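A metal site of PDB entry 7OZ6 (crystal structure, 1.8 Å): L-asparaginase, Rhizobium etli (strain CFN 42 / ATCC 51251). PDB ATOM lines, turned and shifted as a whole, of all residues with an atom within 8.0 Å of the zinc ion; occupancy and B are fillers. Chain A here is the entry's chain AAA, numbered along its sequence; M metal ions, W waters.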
ATOM      1  N   ARG A  53       7.646 -23.413  -2.009  1.00  0.00           N
ATOM      2  CA  ARG A  53       7.945 -23.844  -0.617  1.00  0.00           C
ATOM      3  C   ARG A  53       9.381 -24.382  -0.504  1.00  0.00           C
ATOM      4  O   ARG A  53      10.277 -23.726  -1.006  1.00  0.00           O
ATOM      5  CB  ARG A  53       6.904 -24.890  -0.176  1.00  0.00           C
ATOM      6  CG  ARG A  53       5.467 -24.461  -0.416  1.00  0.00           C
ATOM      7  CD  ARG A  53       4.938 -23.433   0.597  1.00  0.00           C
ATOM      8  NE  ARG A  53       4.918 -23.985   1.919  1.00  0.00           N
ATOM      9  CZ  ARG A  53       3.994 -24.772   2.376  1.00  0.00           C
ATOM     10  NH1 ARG A  53       2.957 -25.103   1.630  1.00  0.00           N
ATOM     11  NH2 ARG A  53       4.117 -25.225   3.587  1.00  0.00           N
ATOM     12  N   SER A  54       9.599 -25.556   0.101  1.00  0.00           N
ATOM     13  CA  SER A  54      10.964 -26.116   0.233  1.00  0.00           C
ATOM     14  C   SER A  54      11.632 -26.364  -1.121  1.00  0.00           C
ATOM     15  O   SER A  54      12.877 -26.476  -1.130  1.00  0.00           O
ATOM     16  CB  SER A  54      10.994 -27.357   1.017  1.00  0.00           C
ATOM     17  OG  SER A  54      10.644 -27.080   2.332  1.00  0.00           O
ATOM     18  N   LYS A  57      14.573 -24.099  -1.822  1.00  0.00           N
ATOM     19  CA  LYS A  57      15.737 -24.123  -0.897  1.00  0.00           C
ATOM     20  C   LYS A  57      17.069 -23.982  -1.616  1.00  0.00           C
ATOM     21  O   LYS A  57      17.944 -23.243  -1.116  1.00  0.00           O
ATOM     22  CB  LYS A  57      15.690 -25.349   0.007  1.00  0.00           C
ATOM     23  CG  LYS A  57      14.718 -25.175   1.142  1.00  0.00           C
ATOM     24  CD  LYS A  57      14.607 -26.350   2.071  1.00  0.00           C
ATOM     25  CE  LYS A  57      13.697 -25.993   3.212  1.00  0.00           C
ATOM     26  NZ  LYS A  57      13.178 -27.189   3.942  1.00  0.00           N
ATOM     27  N   GLN A  60      17.693 -20.399  -2.016  1.00  0.00           N
ATOM     28  CA  GLN A  60      18.023 -19.788  -0.703  1.00  0.00           C
ATOM     29  C   GLN A  60      19.444 -20.164  -0.316  1.00  0.00           C
ATOM     30  O   GLN A  60      20.149 -19.313   0.256  1.00  0.00           O
ATOM     31  CB  GLN A  60      16.982 -20.199   0.361  1.00  0.00           C
ATOM     32  CG  GLN A  60      15.604 -19.640   0.059  1.00  0.00           C
ATOM     33  CD  GLN A  60      14.458 -20.404   0.677  1.00  0.00           C
ATOM     34  OE1 GLN A  60      14.280 -21.598   0.448  1.00  0.00           O
ATOM     35  NE2 GLN A  60      13.659 -19.706   1.463  1.00  0.00           N
ATOM     36  N   MET A  83      21.262 -27.401   4.291  1.00  0.00           N
ATOM     37  CA  MET A  83      20.641 -26.105   3.965  1.00  0.00           C
ATOM     38  C   MET A  83      19.568 -26.310   2.892  1.00  0.00           C
ATOM     39  O   MET A  83      18.540 -25.611   2.923  1.00  0.00           O
ATOM     40  CB  MET A  83      21.652 -25.096   3.427  1.00  0.00           C
ATOM     41  CG  MET A  83      22.707 -24.732   4.402  1.00  0.00           C
ATOM     42  SD  MET A  83      23.797 -23.475   3.622  1.00  0.00           S
ATOM     43  CE  MET A  83      25.034 -23.424   4.911  1.00  0.00           C
ATOM     44  N   ALA A  85      17.726 -28.936   2.546  1.00  0.00           N
ATOM     45  CA  ALA A  85      16.921 -30.082   3.044  1.00  0.00           C
ATOM     46  C   ALA A  85      15.514 -29.683   3.501  1.00  0.00           C
ATOM     47  O   ALA A  85      15.318 -28.577   4.070  1.00  0.00           O
ATOM     48  CB  ALA A  85      17.602 -30.750   4.198  1.00  0.00           C
ATOM     49  N   SER A  86      14.555 -30.611   3.294  1.00  0.00           N
ATOM     50  CA  SER A  86      13.354 -30.855   4.147  1.00  0.00           C
ATOM     51  C   SER A  86      13.590 -32.170   4.883  1.00  0.00           C
ATOM     52  O   SER A  86      13.075 -33.265   4.441  1.00  0.00           O
ATOM     53  CB  SER A  86      12.067 -30.888   3.354  1.00  0.00           C
ATOM     54  OG  SER A  86      11.894 -29.705   2.605  1.00  0.00           O
ATOM     55  N   CYS A 113      12.709 -20.742  13.601  1.00  0.00           N
ATOM     56  CA  CYS A 113      11.803 -21.831  13.117  1.00  0.00           C
ATOM     57  C   CYS A 113      11.311 -22.602  14.332  1.00  0.00           C
ATOM     58  O   CYS A 113      11.989 -22.550  15.342  1.00  0.00           O
ATOM     59  CB  CYS A 113      12.491 -22.793  12.170  1.00  0.00           C
ATOM     60  SG  CYS A 113      14.119 -23.349  12.754  1.00  0.00           S
ATOM     61  N   SER A 139      13.356 -28.673  13.317  1.00  0.00           N
ATOM     62  CA  SER A 139      12.688 -28.195  12.064  1.00  0.00           C
ATOM     63  C   SER A 139      13.299 -28.862  10.834  1.00  0.00           C
ATOM     64  O   SER A 139      14.567 -28.898  10.742  1.00  0.00           O
ATOM     65  CB  SER A 139      12.810 -26.719  11.971  1.00  0.00           C
ATOM     66  OG  SER A 139      12.242 -26.265  10.771  1.00  0.00           O
ATOM     67  N   ASN A 140      12.454 -29.344   9.896  1.00  0.00           N
ATOM     68  CA  ASN A 140      12.906 -29.865   8.584  1.00  0.00           C
ATOM     69  C   ASN A 140      13.744 -28.818   7.844  1.00  0.00           C
ATOM     70  O   ASN A 140      14.583 -29.217   6.983  1.00  0.00           O
ATOM     71  CB  ASN A 140      11.703 -30.334   7.744  1.00  0.00           C
ATOM     72  CG  ASN A 140      10.974 -29.161   7.107  1.00  0.00           C
ATOM     73  OD1 ASN A 140      11.177 -28.861   5.938  1.00  0.00           O
ATOM     74  ND2 ASN A 140      10.146 -28.494   7.868  1.00  0.00           N
ATOM     75  N   CYS A 141      13.568 -27.517   8.185  1.00  0.00           N
ATOM     76  CA  CYS A 141      14.244 -26.364   7.570  1.00  0.00           C
ATOM     77  C   CYS A 141      15.364 -25.846   8.478  1.00  0.00           C
ATOM     78  O   CYS A 141      15.867 -24.731   8.175  1.00  0.00           O
ATOM     79  CB  CYS A 141      13.300 -25.200   7.322  1.00  0.00           C
ATOM     80  SG  CYS A 141      11.875 -25.665   6.296  1.00  0.00           S
ATOM     81  N   SER A 142      15.775 -26.588   9.503  1.00  0.00           N
ATOM     82  CA  SER A 142      16.832 -26.130  10.470  1.00  0.00           C
ATOM     83  C   SER A 142      18.123 -25.726   9.742  1.00  0.00           C
ATOM     84  O   SER A 142      18.718 -24.692  10.112  1.00  0.00           O
ATOM     85  CB  SER A 142      17.116 -27.177  11.534  1.00  0.00           C
ATOM     86  OG  SER A 142      17.671 -28.365  11.001  1.00  0.00           O
ATOM     87  N   LYS A 144      18.525 -24.643   6.680  1.00  0.00           N
ATOM     88  CA  LYS A 144      18.311 -23.368   6.000  1.00  0.00           C
ATOM     89  C   LYS A 144      18.442 -22.256   7.041  1.00  0.00           C
ATOM     90  O   LYS A 144      19.094 -21.188   6.714  1.00  0.00           O
ATOM     91  CB  LYS A 144      16.968 -23.388   5.271  1.00  0.00           C
ATOM     92  CG  LYS A 144      16.559 -22.047   4.701  1.00  0.00           C
ATOM     93  CD  LYS A 144      15.198 -22.089   4.004  1.00  0.00           C
ATOM     94  CE  LYS A 144      14.105 -22.701   4.840  1.00  0.00           C
ATOM     95  NZ  LYS A 144      12.847 -22.653   4.082  1.00  0.00           N
ATOM     96  N   HIS A 145      17.870 -22.457   8.220  1.00  0.00           N
ATOM     97  CA  HIS A 145      17.821 -21.393   9.246  1.00  0.00           C
ATOM     98  C   HIS A 145      19.251 -21.119   9.733  1.00  0.00           C
ATOM     99  O   HIS A 145      19.586 -19.943   9.830  1.00  0.00           O
ATOM    100  CB  HIS A 145      16.827 -21.731  10.333  1.00  0.00           C
ATOM    101  CG  HIS A 145      15.444 -21.371   9.947  1.00  0.00           C
ATOM    102  ND1 HIS A 145      14.821 -20.234  10.405  1.00  0.00           N
ATOM    103  CD2 HIS A 145      14.570 -21.983   9.118  1.00  0.00           C
ATOM    104  CE1 HIS A 145      13.626 -20.159   9.888  1.00  0.00           C
ATOM    105  NE2 HIS A 145      13.453 -21.224   9.095  1.00  0.00           N
ATOM    106  N   ASP A 193       6.282 -19.125   5.326  1.00  0.00           N
ATOM    107  CA  ASP A 193       6.346 -20.606   5.315  1.00  0.00           C
ATOM    108  C   ASP A 193       6.010 -21.200   6.717  1.00  0.00           C
ATOM    109  O   ASP A 193       5.885 -20.464   7.704  1.00  0.00           O
ATOM    110  CB  ASP A 193       7.722 -21.049   4.829  1.00  0.00           C
ATOM    111  CG  ASP A 193       7.667 -22.190   3.825  1.00  0.00           C
ATOM    112  OD1 ASP A 193       6.740 -23.007   3.967  1.00  0.00           O
ATOM    113  OD2 ASP A 193       8.554 -22.231   2.935  1.00  0.00           O
ATOM    114  N   GLY A 194       5.885 -22.526   6.817  1.00  0.00           N
ATOM    115  CA  GLY A 194       5.708 -23.236   8.103  1.00  0.00           C
ATOM    116  C   GLY A 194       6.877 -22.940   9.047  1.00  0.00           C
ATOM    117  O   GLY A 194       6.639 -22.881  10.279  1.00  0.00           O
ATOM    118  N   CYS A 195       8.082 -22.733   8.503  1.00  0.00           N
ATOM    119  CA  CYS A 195       9.327 -22.566   9.289  1.00  0.00           C
ATOM    120  C   CYS A 195       9.510 -21.089   9.626  1.00  0.00           C
ATOM    121  O   CYS A 195      10.536 -20.762  10.211  1.00  0.00           O
ATOM    122  CB  CYS A 195      10.551 -23.023   8.534  1.00  0.00           C
ATOM    123  SG  CYS A 195      10.819 -22.095   7.001  1.00  0.00           S
ATOM    124  N   ASN A 196       8.572 -20.242   9.228  1.00  0.00           N
ATOM    125  CA  ASN A 196       8.528 -18.813   9.604  1.00  0.00           C
ATOM    126  C   ASN A 196       9.470 -17.942   8.756  1.00  0.00           C
ATOM    127  O   ASN A 196       9.791 -16.827   9.194  1.00  0.00           O
ATOM    128  CB  ASN A 196       8.902 -18.631  11.076  1.00  0.00           C
ATOM    129  CG  ASN A 196       8.187 -17.470  11.723  1.00  0.00           C
ATOM    130  OD1 ASN A 196       7.071 -17.095  11.325  1.00  0.00           O
ATOM    131  ND2 ASN A 196       8.813 -16.896  12.733  1.00  0.00           N
ATOM    132  N   LEU A 197       9.913 -18.404   7.590  1.00  0.00           N
ATOM    133  CA  LEU A 197      10.712 -17.590   6.638  1.00  0.00           C
ATOM    134  C   LEU A 197       9.775 -17.076   5.560  1.00  0.00           C
ATOM    135  O   LEU A 197       8.690 -17.650   5.313  1.00  0.00           O
ATOM    136  CB  LEU A 197      11.818 -18.434   6.022  1.00  0.00           C
ATOM    137  CG  LEU A 197      13.040 -18.682   6.920  1.00  0.00           C
ATOM    138  CD1 LEU A 197      14.054 -19.610   6.248  1.00  0.00           C
ATOM    139  CD2 LEU A 197      13.706 -17.379   7.306  1.00  0.00           C
ATOM    140  N   PRO A 198      10.180 -16.012   4.821  1.00  0.00           N
ATOM    141  CA  PRO A 198       9.471 -15.606   3.625  1.00  0.00           C
ATOM    142  C   PRO A 198       9.576 -16.802   2.659  1.00  0.00           C
ATOM    143  O   PRO A 198      10.615 -17.448   2.646  1.00  0.00           O
ATOM    144  CB  PRO A 198      10.279 -14.403   3.092  1.00  0.00           C
ATOM    145  CG  PRO A 198      11.042 -13.951   4.285  1.00  0.00           C
ATOM    146  CD  PRO A 198      11.363 -15.188   5.077  1.00  0.00           C
ATOM    147  N   THR A 199       8.548 -17.033   1.882  1.00  0.00           N
ATOM    148  CA  THR A 199       8.543 -18.124   0.879  1.00  0.00           C
ATOM    149  C   THR A 199       7.940 -17.621  -0.424  1.00  0.00           C
ATOM    150  O   THR A 199       6.896 -16.954  -0.424  1.00  0.00           O
ATOM    151  CB  THR A 199       7.802 -19.340   1.495  1.00  0.00           C
ATOM    152  OG1 THR A 199       8.113 -20.475   0.667  1.00  0.00           O
ATOM    153  CG2 THR A 199       6.305 -19.122   1.621  1.00  0.00           C
HETATM  154 ZN    ZN M   1      11.357 -23.585   5.413  1.00  0.00          ZN
HETATM  155  O   HOH W   1      10.167 -24.367   3.779  1.00  0.00           O
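The side-chain sulfur of Cys 141 lies close to the side-chain amide oxygen of Asn 140. N of Cys 141 sits close to OG of Ser 139 (3.2 Å). The side-chain carboxylate of Asp 193 lies within hydrogen-bond range of the side-chain hydroxyl of Thr 199. The side-chain carboxylate (OD1) of Asp 193 lies within salt-bridge range of the guanidinium group (NE) of Arg 53 (2.9 Å). The backbone carbonyl oxygen (O) of Cys 195 is in hydrogen-bond range of a ring nitrogen (NE2) of His 145 (3.2 Å). The side-chain amino group of Lys 57 sits close to the side-chain sulfur of Cys 141 (3.1 Å).
Residues that only touch the zinc ion: Asp 193 (3.98 Å). Within 4 Å of the zinc ion: Cys 141, Lys 144, Asp 193 and Cys 195. The nearest printed residue that does not touch the zinc ion is Lys 57 (4.01 Å).
The zinc ion is bound by water W1 (2.2 Å), the side-chain amino group of Lys 144 (2.2 Å), the side-chain sulfur of Cys 195 (2.2 Å) and the side-chain sulfur of Cys 141 (2.3 Å).
Water W1 lies within hydrogen-bond range of OD2 of Asp 193 (2.8 Å) and OG of Ser 54 (3.1 Å).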
